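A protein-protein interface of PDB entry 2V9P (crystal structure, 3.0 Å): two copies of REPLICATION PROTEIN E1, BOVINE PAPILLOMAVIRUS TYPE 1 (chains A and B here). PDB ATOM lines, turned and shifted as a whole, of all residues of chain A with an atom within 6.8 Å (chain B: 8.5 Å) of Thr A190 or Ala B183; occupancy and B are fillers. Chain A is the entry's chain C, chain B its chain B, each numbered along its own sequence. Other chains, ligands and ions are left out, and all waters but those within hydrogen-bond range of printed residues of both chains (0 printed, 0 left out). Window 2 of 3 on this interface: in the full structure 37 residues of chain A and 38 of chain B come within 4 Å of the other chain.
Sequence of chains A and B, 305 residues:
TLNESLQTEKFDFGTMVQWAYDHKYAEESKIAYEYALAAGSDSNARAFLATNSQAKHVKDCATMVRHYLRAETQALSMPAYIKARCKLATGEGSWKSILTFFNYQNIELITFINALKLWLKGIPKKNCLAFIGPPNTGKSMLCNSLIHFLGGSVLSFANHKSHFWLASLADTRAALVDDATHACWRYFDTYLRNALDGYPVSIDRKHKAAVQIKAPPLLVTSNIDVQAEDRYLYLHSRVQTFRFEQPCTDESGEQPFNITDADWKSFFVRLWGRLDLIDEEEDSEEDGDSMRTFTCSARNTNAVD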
ATOM      1  N   TRP A 185     -14.424 -29.542  12.240  1.00  0.00           N
ATOM      2  CA  TRP A 185     -14.085 -28.267  11.634  1.00  0.00           C
ATOM      3  C   TRP A 185     -15.102 -27.195  12.013  1.00  0.00           C
ATOM      4  O   TRP A 185     -14.719 -26.067  12.345  1.00  0.00           O
ATOM      5  CB  TRP A 185     -13.956 -28.384  10.114  1.00  0.00           C
ATOM      6  CG  TRP A 185     -12.674 -29.016   9.672  1.00  0.00           C
ATOM      7  CD1 TRP A 185     -12.540 -30.131   8.904  1.00  0.00           C
ATOM      8  CD2 TRP A 185     -11.338 -28.575   9.972  1.00  0.00           C
ATOM      9  NE1 TRP A 185     -11.210 -30.412   8.695  1.00  0.00           N
ATOM     10  CE2 TRP A 185     -10.452 -29.474   9.343  1.00  0.00           C
ATOM     11  CE3 TRP A 185     -10.804 -27.504  10.707  1.00  0.00           C
ATOM     12  CZ2 TRP A 185      -9.060 -29.343   9.437  1.00  0.00           C
ATOM     13  CZ3 TRP A 185      -9.419 -27.379  10.801  1.00  0.00           C
ATOM     14  CH2 TRP A 185      -8.567 -28.291  10.171  1.00  0.00           C
ATOM     15  N   ARG A 186     -16.387 -27.557  11.995  1.00  0.00           N
ATOM     16  CA  ARG A 186     -17.445 -26.598  12.306  1.00  0.00           C
ATOM     17  C   ARG A 186     -17.353 -26.068  13.723  1.00  0.00           C
ATOM     18  O   ARG A 186     -17.447 -24.857  13.945  1.00  0.00           O
ATOM     19  CB  ARG A 186     -18.835 -27.159  12.028  1.00  0.00           C
ATOM     20  CG  ARG A 186     -19.539 -26.406  10.926  1.00  0.00           C
ATOM     21  CD  ARG A 186     -20.950 -26.929  10.671  1.00  0.00           C
ATOM     22  NE  ARG A 186     -20.981 -28.203   9.945  1.00  0.00           N
ATOM     23  CZ  ARG A 186     -21.140 -29.404  10.504  1.00  0.00           C
ATOM     24  NH1 ARG A 186     -21.278 -29.537  11.824  1.00  0.00           N
ATOM     25  NH2 ARG A 186     -21.153 -30.484   9.731  1.00  0.00           N
ATOM     26  N   TYR A 187     -17.147 -26.972  14.675  1.00  0.00           N
ATOM     27  CA  TYR A 187     -16.994 -26.569  16.061  1.00  0.00           C
ATOM     28  C   TYR A 187     -15.844 -25.566  16.190  1.00  0.00           C
ATOM     29  O   TYR A 187     -16.019 -24.489  16.761  1.00  0.00           O
ATOM     30  CB  TYR A 187     -16.786 -27.779  16.976  1.00  0.00           C
ATOM     31  CG  TYR A 187     -16.723 -27.417  18.449  1.00  0.00           C
ATOM     32  CD1 TYR A 187     -17.861 -27.449  19.236  1.00  0.00           C
ATOM     33  CD2 TYR A 187     -15.523 -27.024  19.048  1.00  0.00           C
ATOM     34  CE1 TYR A 187     -17.824 -27.105  20.582  1.00  0.00           C
ATOM     35  CE2 TYR A 187     -15.462 -26.679  20.395  1.00  0.00           C
ATOM     36  CZ  TYR A 187     -16.623 -26.720  21.166  1.00  0.00           C
ATOM     37  OH  TYR A 187     -16.600 -26.389  22.521  1.00  0.00           O
ATOM     38  N   PHE A 188     -14.685 -25.911  15.641  1.00  0.00           N
ATOM     39  CA  PHE A 188     -13.565 -24.985  15.619  1.00  0.00           C
ATOM     40  C   PHE A 188     -13.894 -23.652  14.993  1.00  0.00           C
ATOM     41  O   PHE A 188     -13.577 -22.620  15.576  1.00  0.00           O
ATOM     42  CB  PHE A 188     -12.366 -25.595  14.924  1.00  0.00           C
ATOM     43  CG  PHE A 188     -11.604 -26.516  15.797  1.00  0.00           C
ATOM     44  CD1 PHE A 188     -10.770 -26.013  16.788  1.00  0.00           C
ATOM     45  CD2 PHE A 188     -11.743 -27.893  15.661  1.00  0.00           C
ATOM     46  CE1 PHE A 188     -10.076 -26.863  17.623  1.00  0.00           C
ATOM     47  CE2 PHE A 188     -11.047 -28.756  16.490  1.00  0.00           C
ATOM     48  CZ  PHE A 188     -10.214 -28.239  17.477  1.00  0.00           C
ATOM     49  N   ASP A 189     -14.529 -23.675  13.822  1.00  0.00           N
ATOM     50  CA  ASP A 189     -14.934 -22.450  13.146  1.00  0.00           C
ATOM     51  C   ASP A 189     -15.814 -21.584  14.052  1.00  0.00           C
ATOM     52  O   ASP A 189     -15.569 -20.385  14.205  1.00  0.00           O
ATOM     53  CB  ASP A 189     -15.653 -22.769  11.829  1.00  0.00           C
ATOM     54  CG  ASP A 189     -16.073 -21.517  11.060  1.00  0.00           C
ATOM     55  OD1 ASP A 189     -17.234 -21.469  10.588  1.00  0.00           O
ATOM     56  OD2 ASP A 189     -15.254 -20.578  10.929  1.00  0.00           O
ATOM     57  N   THR A 190     -16.811 -22.206  14.674  1.00  0.00           N
ATOM     58  CA  THR A 190     -17.783 -21.483  15.477  1.00  0.00           C
ATOM     59  C   THR A 190     -17.206 -20.943  16.785  1.00  0.00           C
ATOM     60  O   THR A 190     -17.478 -19.801  17.157  1.00  0.00           O
ATOM     61  CB  THR A 190     -19.004 -22.369  15.794  1.00  0.00           C
ATOM     62  OG1 THR A 190     -19.394 -23.091  14.622  1.00  0.00           O
ATOM     63  CG2 THR A 190     -20.184 -21.530  16.282  1.00  0.00           C
ATOM     64  N   TYR A 191     -16.409 -21.759  17.472  1.00  0.00           N
ATOM     65  CA  TYR A 191     -16.063 -21.484  18.869  1.00  0.00           C
ATOM     66  C   TYR A 191     -14.606 -21.180  19.171  1.00  0.00           C
ATOM     67  O   TYR A 191     -14.306 -20.658  20.241  1.00  0.00           O
ATOM     68  CB  TYR A 191     -16.481 -22.662  19.738  1.00  0.00           C
ATOM     69  CG  TYR A 191     -17.963 -22.898  19.771  1.00  0.00           C
ATOM     70  CD1 TYR A 191     -18.534 -23.929  19.035  1.00  0.00           C
ATOM     71  CD2 TYR A 191     -18.798 -22.089  20.532  1.00  0.00           C
ATOM     72  CE1 TYR A 191     -19.906 -24.152  19.055  1.00  0.00           C
ATOM     73  CE2 TYR A 191     -20.162 -22.300  20.560  1.00  0.00           C
ATOM     74  CZ  TYR A 191     -20.713 -23.335  19.824  1.00  0.00           C
ATOM     75  OH  TYR A 191     -22.073 -23.551  19.855  1.00  0.00           O
ATOM     76  N   LEU A 192     -13.707 -21.502  18.248  1.00  0.00           N
ATOM     77  CA  LEU A 192     -12.295 -21.576  18.594  1.00  0.00           C
ATOM     78  C   LEU A 192     -11.325 -20.915  17.628  1.00  0.00           C
ATOM     79  O   LEU A 192     -10.151 -21.284  17.580  1.00  0.00           O
ATOM     80  CB  LEU A 192     -11.896 -23.036  18.794  1.00  0.00           C
ATOM     81  CG  LEU A 192     -12.429 -23.703  20.056  1.00  0.00           C
ATOM     82  CD1 LEU A 192     -12.217 -25.150  19.999  1.00  0.00           C
ATOM     83  CD2 LEU A 192     -11.690 -23.208  21.236  1.00  0.00           C
ATOM     84  N   ARG A 193     -11.795 -19.927  16.876  1.00  0.00           N
ATOM     85  CA  ARG A 193     -10.905 -19.215  15.961  1.00  0.00           C
ATOM     86  C   ARG A 193      -9.720 -18.607  16.702  1.00  0.00           C
ATOM     87  O   ARG A 193      -8.577 -18.718  16.259  1.00  0.00           O
ATOM     88  CB  ARG A 193     -11.658 -18.135  15.219  1.00  0.00           C
ATOM     89  CG  ARG A 193     -12.702 -18.680  14.306  1.00  0.00           C
ATOM     90  CD  ARG A 193     -13.347 -17.541  13.585  1.00  0.00           C
ATOM     91  NE  ARG A 193     -14.415 -17.974  12.700  1.00  0.00           N
ATOM     92  CZ  ARG A 193     -15.297 -17.145  12.163  1.00  0.00           C
ATOM     93  NH1 ARG A 193     -15.235 -15.843  12.429  1.00  0.00           N
ATOM     94  NH2 ARG A 193     -16.241 -17.619  11.368  1.00  0.00           N
ATOM     95  N   LEU A 235     -11.501 -19.918   8.127  1.00  0.00           N
ATOM     96  CA  LEU A 235     -10.385 -20.729   8.597  1.00  0.00           C
ATOM     97  C   LEU A 235      -9.204 -20.681   7.646  1.00  0.00           C
ATOM     98  O   LEU A 235      -8.091 -21.054   8.020  1.00  0.00           O
ATOM     99  CB  LEU A 235     -10.803 -22.186   8.759  1.00  0.00           C
ATOM    100  CG  LEU A 235     -11.855 -22.586   9.790  1.00  0.00           C
ATOM    101  CD1 LEU A 235     -12.072 -24.088   9.699  1.00  0.00           C
ATOM    102  CD2 LEU A 235     -11.431 -22.193  11.196  1.00  0.00           C
ATOM    103  N   SER B 156     -14.359 -16.997  26.525  1.00  0.00           N
ATOM    104  CA  SER B 156     -14.313 -18.035  25.517  1.00  0.00           C
ATOM    105  C   SER B 156     -15.694 -18.619  25.274  1.00  0.00           C
ATOM    106  O   SER B 156     -16.144 -19.502  25.994  1.00  0.00           O
ATOM    107  CB  SER B 156     -13.261 -19.099  25.868  1.00  0.00           C
ATOM    108  OG  SER B 156     -11.942 -18.599  25.604  1.00  0.00           O
ATOM    109  N   PHE B 157     -16.366 -18.102  24.248  1.00  0.00           N
ATOM    110  CA  PHE B 157     -17.707 -18.549  23.902  1.00  0.00           C
ATOM    111  C   PHE B 157     -17.761 -20.065  23.720  1.00  0.00           C
ATOM    112  O   PHE B 157     -18.831 -20.656  23.806  1.00  0.00           O
ATOM    113  CB  PHE B 157     -18.190 -17.822  22.647  1.00  0.00           C
ATOM    114  CG  PHE B 157     -19.585 -18.168  22.243  1.00  0.00           C
ATOM    115  CD1 PHE B 157     -20.640 -17.909  23.099  1.00  0.00           C
ATOM    116  CD2 PHE B 157     -19.847 -18.750  21.000  1.00  0.00           C
ATOM    117  CE1 PHE B 157     -21.940 -18.230  22.737  1.00  0.00           C
ATOM    118  CE2 PHE B 157     -21.150 -19.083  20.624  1.00  0.00           C
ATOM    119  CZ  PHE B 157     -22.198 -18.818  21.499  1.00  0.00           C
ATOM    120  N   ALA B 158     -16.600 -20.683  23.490  1.00  0.00           N
ATOM    121  CA  ALA B 158     -16.475 -22.136  23.383  1.00  0.00           C
ATOM    122  C   ALA B 158     -16.988 -22.828  24.634  1.00  0.00           C
ATOM    123  O   ALA B 158     -17.437 -23.969  24.574  1.00  0.00           O
ATOM    124  CB  ALA B 158     -15.026 -22.528  23.127  1.00  0.00           C
ATOM    125  N   HIS B 160     -19.515 -21.594  26.570  1.00  0.00           N
ATOM    126  CA  HIS B 160     -20.774 -20.948  26.938  1.00  0.00           C
ATOM    127  C   HIS B 160     -21.791 -21.926  27.532  1.00  0.00           C
ATOM    128  O   HIS B 160     -22.701 -21.508  28.234  1.00  0.00           O
ATOM    129  CB  HIS B 160     -21.381 -20.211  25.747  1.00  0.00           C
ATOM    130  CG  HIS B 160     -22.097 -21.115  24.800  1.00  0.00           C
ATOM    131  ND1 HIS B 160     -21.483 -21.678  23.705  1.00  0.00           N
ATOM    132  CD2 HIS B 160     -23.361 -21.596  24.813  1.00  0.00           C
ATOM    133  CE1 HIS B 160     -22.343 -22.459  23.077  1.00  0.00           C
ATOM    134  NE2 HIS B 160     -23.489 -22.428  23.731  1.00  0.00           N
ATOM    135  N   VAL B 177     -14.423 -10.511  23.620  1.00  0.00           N
ATOM    136  CA  VAL B 177     -14.880 -11.667  22.868  1.00  0.00           C
ATOM    137  C   VAL B 177     -14.303 -11.585  21.457  1.00  0.00           C
ATOM    138  O   VAL B 177     -14.636 -10.679  20.698  1.00  0.00           O
ATOM    139  CB  VAL B 177     -16.416 -11.757  22.870  1.00  0.00           C
ATOM    140  CG1 VAL B 177     -16.909 -12.845  21.924  1.00  0.00           C
ATOM    141  CG2 VAL B 177     -16.886 -12.059  24.266  1.00  0.00           C
ATOM    142  N   ASP B 178     -13.422 -12.532  21.138  1.00  0.00           N
ATOM    143  CA  ASP B 178     -12.631 -12.506  19.916  1.00  0.00           C
ATOM    144  C   ASP B 178     -13.264 -13.406  18.878  1.00  0.00           C
ATOM    145  O   ASP B 178     -13.496 -14.580  19.154  1.00  0.00           O
ATOM    146  CB  ASP B 178     -11.206 -12.987  20.208  1.00  0.00           C
ATOM    147  CG  ASP B 178     -10.173 -12.377  19.271  1.00  0.00           C
ATOM    148  OD1 ASP B 178     -10.275 -11.164  18.983  1.00  0.00           O
ATOM    149  OD2 ASP B 178      -9.254 -13.105  18.825  1.00  0.00           O
ATOM    150  N   ASP B 179     -13.532 -12.856  17.689  1.00  0.00           N
ATOM    151  CA  ASP B 179     -14.205 -13.569  16.582  1.00  0.00           C
ATOM    152  C   ASP B 179     -15.589 -14.066  16.964  1.00  0.00           C
ATOM    153  O   ASP B 179     -15.802 -15.270  17.132  1.00  0.00           O
ATOM    154  CB  ASP B 179     -13.359 -14.734  16.053  1.00  0.00           C
ATOM    155  CG  ASP B 179     -12.383 -14.308  14.973  1.00  0.00           C
ATOM    156  OD1 ASP B 179     -12.825 -14.143  13.800  1.00  0.00           O
ATOM    157  OD2 ASP B 179     -11.176 -14.153  15.305  1.00  0.00           O
ATOM    158  N   ALA B 180     -16.525 -13.136  17.116  1.00  0.00           N
ATOM    159  CA  ALA B 180     -17.910 -13.500  17.371  1.00  0.00           C
ATOM    160  C   ALA B 180     -18.528 -14.031  16.083  1.00  0.00           C
ATOM    161  O   ALA B 180     -18.638 -13.313  15.094  1.00  0.00           O
ATOM    162  CB  ALA B 180     -18.683 -12.317  17.898  1.00  0.00           C
ATOM    163  N   THR B 181     -18.894 -15.304  16.092  1.00  0.00           N
ATOM    164  CA  THR B 181     -19.569 -15.902  14.952  1.00  0.00           C
ATOM    165  C   THR B 181     -21.059 -15.598  15.067  1.00  0.00           C
ATOM    166  O   THR B 181     -21.473 -14.889  15.986  1.00  0.00           O
ATOM    167  CB  THR B 181     -19.334 -17.412  14.912  1.00  0.00           C
ATOM    168  OG1 THR B 181     -19.749 -17.986  16.151  1.00  0.00           O
ATOM    169  CG2 THR B 181     -17.859 -17.711  14.703  1.00  0.00           C
ATOM    170  N   HIS B 182     -21.864 -16.113  14.141  1.00  0.00           N
ATOM    171  CA  HIS B 182     -23.314 -15.906  14.203  1.00  0.00           C
ATOM    172  C   HIS B 182     -23.927 -16.533  15.453  1.00  0.00           C
ATOM    173  O   HIS B 182     -24.791 -15.935  16.103  1.00  0.00           O
ATOM    174  CB  HIS B 182     -23.995 -16.421  12.946  1.00  0.00           C
ATOM    175  CG  HIS B 182     -24.009 -15.431  11.828  1.00  0.00           C
ATOM    176  ND1 HIS B 182     -24.723 -14.254  11.890  1.00  0.00           N
ATOM    177  CD2 HIS B 182     -23.404 -15.442  10.615  1.00  0.00           C
ATOM    178  CE1 HIS B 182     -24.559 -13.582  10.764  1.00  0.00           C
ATOM    179  NE2 HIS B 182     -23.764 -14.281   9.973  1.00  0.00           N
ATOM    180  N   ALA B 183     -23.460 -17.732  15.790  1.00  0.00           N
ATOM    181  CA  ALA B 183     -23.853 -18.391  17.031  1.00  0.00           C
ATOM    182  C   ALA B 183     -23.548 -17.499  18.224  1.00  0.00           C
ATOM    183  O   ALA B 183     -24.372 -17.354  19.126  1.00  0.00           O
ATOM    184  CB  ALA B 183     -23.146 -19.725  17.180  1.00  0.00           C
ATOM    185  N   CYS B 184     -22.371 -16.890  18.213  1.00  0.00           N
ATOM    186  CA  CYS B 184     -21.975 -15.999  19.275  1.00  0.00           C
ATOM    187  C   CYS B 184     -22.895 -14.786  19.378  1.00  0.00           C
ATOM    188  O   CYS B 184     -23.438 -14.495  20.444  1.00  0.00           O
ATOM    189  CB  CYS B 184     -20.525 -15.579  19.079  1.00  0.00           C
ATOM    190  SG  CYS B 184     -19.872 -14.660  20.470  1.00  0.00           S
ATOM    191  N   TRP B 185     -23.093 -14.097  18.263  1.00  0.00           N
ATOM    192  CA  TRP B 185     -23.943 -12.926  18.263  1.00  0.00           C
ATOM    193  C   TRP B 185     -25.357 -13.247  18.728  1.00  0.00           C
ATOM    194  O   TRP B 185     -25.954 -12.481  19.486  1.00  0.00           O
ATOM    195  CB  TRP B 185     -23.975 -12.279  16.889  1.00  0.00           C
ATOM    196  CG  TRP B 185     -22.742 -11.460  16.551  1.00  0.00           C
ATOM    197  CD1 TRP B 185     -21.891 -11.666  15.505  1.00  0.00           C
ATOM    198  CD2 TRP B 185     -22.237 -10.304  17.250  1.00  0.00           C
ATOM    199  NE1 TRP B 185     -20.893 -10.717  15.506  1.00  0.00           N
ATOM    200  CE2 TRP B 185     -21.085  -9.872  16.564  1.00  0.00           C
ATOM    201  CE3 TRP B 185     -22.651  -9.593  18.382  1.00  0.00           C
ATOM    202  CZ2 TRP B 185     -20.346  -8.770  16.970  1.00  0.00           C
ATOM    203  CZ3 TRP B 185     -21.907  -8.500  18.788  1.00  0.00           C
ATOM    204  CH2 TRP B 185     -20.768  -8.101  18.085  1.00  0.00           C
ATOM    205  N   ARG B 186     -25.895 -14.381  18.292  1.00  0.00           N
ATOM    206  CA  ARG B 186     -27.238 -14.743  18.715  1.00  0.00           C
ATOM    207  C   ARG B 186     -27.334 -14.965  20.212  1.00  0.00           C
ATOM    208  O   ARG B 186     -28.274 -14.486  20.848  1.00  0.00           O
ATOM    209  CB  ARG B 186     -27.799 -15.916  17.928  1.00  0.00           C
ATOM    210  CG  ARG B 186     -28.880 -15.459  16.937  1.00  0.00           C
ATOM    211  CD  ARG B 186     -29.325 -16.552  15.973  1.00  0.00           C
ATOM    212  NE  ARG B 186     -28.619 -17.789  16.262  1.00  0.00           N
ATOM    213  CZ  ARG B 186     -27.715 -18.423  15.516  1.00  0.00           C
ATOM    214  NH1 ARG B 186     -27.194 -19.531  16.024  1.00  0.00           N
ATOM    215  NH2 ARG B 186     -27.339 -18.003  14.306  1.00  0.00           N
ATOM    216  N   TYR B 187     -26.355 -15.670  20.778  1.00  0.00           N
ATOM    217  CA  TYR B 187     -26.359 -15.918  22.217  1.00  0.00           C
ATOM    218  C   TYR B 187     -26.395 -14.594  22.954  1.00  0.00           C
ATOM    219  O   TYR B 187     -27.210 -14.401  23.863  1.00  0.00           O
ATOM    220  CB  TYR B 187     -25.152 -16.732  22.664  1.00  0.00           C
ATOM    221  CG  TYR B 187     -25.175 -17.051  24.141  1.00  0.00           C
ATOM    222  CD1 TYR B 187     -25.745 -18.229  24.608  1.00  0.00           C
ATOM    223  CD2 TYR B 187     -24.638 -16.166  25.072  1.00  0.00           C
ATOM    224  CE1 TYR B 187     -25.771 -18.525  25.965  1.00  0.00           C
ATOM    225  CE2 TYR B 187     -24.655 -16.446  26.424  1.00  0.00           C
ATOM    226  CZ  TYR B 187     -25.218 -17.630  26.879  1.00  0.00           C
ATOM    227  OH  TYR B 187     -25.222 -17.913  28.249  1.00  0.00           O
ATOM    228  N   PHE B 188     -25.525 -13.681  22.546  1.00  0.00           N
ATOM    229  CA  PHE B 188     -25.515 -12.364  23.137  1.00  0.00           C
ATOM    230  C   PHE B 188     -26.850 -11.657  23.016  1.00  0.00           C
ATOM    231  O   PHE B 188     -27.337 -11.096  23.993  1.00  0.00           O
ATOM    232  CB  PHE B 188     -24.395 -11.527  22.549  1.00  0.00           C
ATOM    233  CG  PHE B 188     -23.079 -11.807  23.178  1.00  0.00           C
ATOM    234  CD1 PHE B 188     -22.823 -11.400  24.486  1.00  0.00           C
ATOM    235  CD2 PHE B 188     -22.102 -12.505  22.484  1.00  0.00           C
ATOM    236  CE1 PHE B 188     -21.616 -11.667  25.086  1.00  0.00           C
ATOM    237  CE2 PHE B 188     -20.885 -12.778  23.080  1.00  0.00           C
ATOM    238  CZ  PHE B 188     -20.643 -12.359  24.387  1.00  0.00           C
ATOM    239  N   ASP B 189     -27.440 -11.711  21.827  1.00  0.00           N
ATOM    240  CA  ASP B 189     -28.733 -11.106  21.571  1.00  0.00           C
ATOM    241  C   ASP B 189     -29.815 -11.659  22.503  1.00  0.00           C
ATOM    242  O   ASP B 189     -30.566 -10.897  23.116  1.00  0.00           O
ATOM    243  CB  ASP B 189     -29.117 -11.317  20.108  1.00  0.00           C
ATOM    244  CG  ASP B 189     -30.435 -10.649  19.736  1.00  0.00           C
ATOM    245  OD1 ASP B 189     -31.128 -11.210  18.866  1.00  0.00           O
ATOM    246  OD2 ASP B 189     -30.775  -9.575  20.288  1.00  0.00           O
ATOM    247  N   THR B 190     -29.872 -12.980  22.626  1.00  0.00           N
ATOM    248  CA  THR B 190     -30.872 -13.636  23.464  1.00  0.00           C
ATOM    249  C   THR B 190     -30.655 -13.453  24.968  1.00  0.00           C
ATOM    250  O   THR B 190     -31.596 -13.172  25.695  1.00  0.00           O
ATOM    251  CB  THR B 190     -30.919 -15.137  23.187  1.00  0.00           C
ATOM    252  OG1 THR B 190     -30.682 -15.386  21.794  1.00  0.00           O
ATOM    253  CG2 THR B 190     -32.271 -15.721  23.620  1.00  0.00           C
ATOM    254  N   TYR B 191     -29.421 -13.607  25.429  1.00  0.00           N
ATOM    255  CA  TYR B 191     -29.182 -13.769  26.849  1.00  0.00           C
ATOM    256  C   TYR B 191     -28.467 -12.627  27.535  1.00  0.00           C
ATOM    257  O   TYR B 191     -28.530 -12.502  28.765  1.00  0.00           O
ATOM    258  CB  TYR B 191     -28.414 -15.068  27.088  1.00  0.00           C
ATOM    259  CG  TYR B 191     -29.207 -16.273  26.662  1.00  0.00           C
ATOM    260  CD1 TYR B 191     -28.965 -16.889  25.443  1.00  0.00           C
ATOM    261  CD2 TYR B 191     -30.231 -16.783  27.464  1.00  0.00           C
ATOM    262  CE1 TYR B 191     -29.715 -17.998  25.036  1.00  0.00           C
ATOM    263  CE2 TYR B 191     -30.976 -17.889  27.070  1.00  0.00           C
ATOM    264  CZ  TYR B 191     -30.714 -18.483  25.852  1.00  0.00           C
ATOM    265  OH  TYR B 191     -31.434 -19.576  25.452  1.00  0.00           O
ATOM    266  N   ILE B 224     -18.691 -10.255  11.162  1.00  0.00           N
ATOM    267  CA  ILE B 224     -20.119  -9.973  10.993  1.00  0.00           C
ATOM    268  C   ILE B 224     -20.468  -8.550  11.414  1.00  0.00           C
ATOM    269  O   ILE B 224     -20.232  -8.143  12.543  1.00  0.00           O
ATOM    270  CB  ILE B 224     -20.986 -10.978  11.781  1.00  0.00           C
ATOM    271  CG1 ILE B 224     -20.831 -12.384  11.198  1.00  0.00           C
ATOM    272  CG2 ILE B 224     -22.445 -10.558  11.765  1.00  0.00           C
ATOM    273  CD1 ILE B 224     -20.935 -13.509  12.220  1.00  0.00           C
ATOM    274  N   ARG B 231     -31.606  -8.857  11.599  1.00  0.00           N
ATOM    275  CA  ARG B 231     -31.892  -9.868  12.603  1.00  0.00           C
ATOM    276  C   ARG B 231     -31.129  -9.634  13.904  1.00  0.00           C
ATOM    277  O   ARG B 231     -31.381 -10.308  14.913  1.00  0.00           O
ATOM    278  CB  ARG B 231     -31.614 -11.256  12.050  1.00  0.00           C
ATOM    279  CG  ARG B 231     -30.170 -11.502  11.669  1.00  0.00           C
ATOM    280  CD  ARG B 231     -30.154 -12.749  10.844  1.00  0.00           C
ATOM    281  NE  ARG B 231     -28.826 -13.260  10.539  1.00  0.00           N
ATOM    282  CZ  ARG B 231     -28.612 -14.427   9.937  1.00  0.00           C
ATOM    283  NH1 ARG B 231     -29.635 -15.206   9.593  1.00  0.00           N
ATOM    284  NH2 ARG B 231     -27.372 -14.819   9.680  1.00  0.00           N
ATOM    285  N   TYR B 232     -30.190  -8.690  13.864  1.00  0.00           N
ATOM    286  CA  TYR B 232     -29.490  -8.245  15.062  1.00  0.00           C
ATOM    287  C   TYR B 232     -29.901  -6.826  15.420  1.00  0.00           C
ATOM    288  O   TYR B 232     -29.128  -6.066  16.014  1.00  0.00           O
ATOM    289  CB  TYR B 232     -27.985  -8.359  14.870  1.00  0.00           C
ATOM    290  CG  TYR B 232     -27.526  -9.783  14.662  1.00  0.00           C
ATOM    291  CD1 TYR B 232     -26.741 -10.126  13.567  1.00  0.00           C
ATOM    292  CD2 TYR B 232     -27.889 -10.796  15.557  1.00  0.00           C
ATOM    293  CE1 TYR B 232     -26.310 -11.439  13.372  1.00  0.00           C
ATOM    294  CE2 TYR B 232     -27.468 -12.115  15.369  1.00  0.00           C
ATOM    295  CZ  TYR B 232     -26.678 -12.429  14.274  1.00  0.00           C
ATOM    296  OH  TYR B 232     -26.259 -13.730  14.080  1.00  0.00           O
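The side-chain hydroxyl (OH) of Tyr A187 is in hydrogen-bond range of the backbone carbonyl oxygen (O) of Ala B158.
The side-chain carboxylate of Asp B179 is in salt-bridge range of the guanidinium group of Arg A193, at 3.3 Å.
The side-chain hydroxyl (OG1) of Thr B181 is in hydrogen-bond range of the backbone carbonyl oxygen (O) of Thr A190 (3.1 Å).
ND1 of His B160 is in hydrogen-bond range of O of Phe B157 (2.8 Å).
O of Arg A186 sits at hydrogen-bond distance from OG1 of Thr A190 (2.7 Å).
The backbone carbonyl oxygen (O) of Phe A188 sits at hydrogen-bond distance from the backbone NH (N) of Arg A193 (3.5 Å).
The guanidinium group (NH2) of Arg A193 lies within salt-bridge range of the side-chain carboxylate (OD2) of Asp A189 (3.2 Å).
Among the printed residues, pairs that only touch across the chains: Asp A189 with Thr B181 (3.6 Å), Thr A190 with Ala B183 (3.6 Å), Tyr A191 with Phe B157 (3.4 Å), Tyr A191 with Ala B158 (3.5 Å), Tyr A191 with His B160 (3.3 Å), Leu A192 with Ala B158 (3.9 Å) and Arg A193 with Thr B181 (3.7 Å).
Thr A190 touches just these residues of chain B: Thr B181 (3.1 Å) and Ala B183 (3.6 Å).
Of the printed residues of chain A, Ala B183 touches Thr A190.
Of chain B, only Thr B181 comes within 4 Å of Asp A189.
Printed residues of chain A within 4 Å of Asp B179: Arg A193 (3.3 Å).
Printed residues of chain B within 4 Å of Tyr A187: Ala B158 (3.3 Å).
Printed residues of chain A within 4 Å of Ala B158: Tyr A187 (3.3 Å), Tyr A191 (3.5 Å) and Leu A192 (3.9 Å).
Printed residues of chain A within 4 Å of Thr B181: Asp A189 (3.6 Å), Thr A190 (3.1 Å) and Arg A193 (3.7 Å).
Printed residues of chain A within 4 Å of Phe B157: Tyr A191.
The nearest residue of chain B that does not touch Thr A190 is Phe B157 (4.6 Å).
The nearest residue of chain A that does not touch Ala B183 is Tyr A191 (4.8 Å).
The nearest printed residue of chain A that does not touch Phe B157 is Thr A190 (4.6 Å).
Printed residues of chain B that touch a printed residue of chain A: Phe B157, Ala B158, His B160, Asp B179, Thr B181 and Ala B183.
Hydrophobic or aromatic side chains of chain A within 4 Å of the printed part of chain B: Tyr A187, Tyr A191 and Leu A192.
Among the printed residues, Asp or Glu carboxylates within 4 Å of a Lys or Arg side-chain nitrogen of the other chain: Arg A193 with Asp B179.
Positions printed for both chains: 185, 186, 187, 188, 189, 190 and 191.
Of the 10 pairs that touch across the chains among the printed residues, none has its exchanged pair printed and touching as well.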
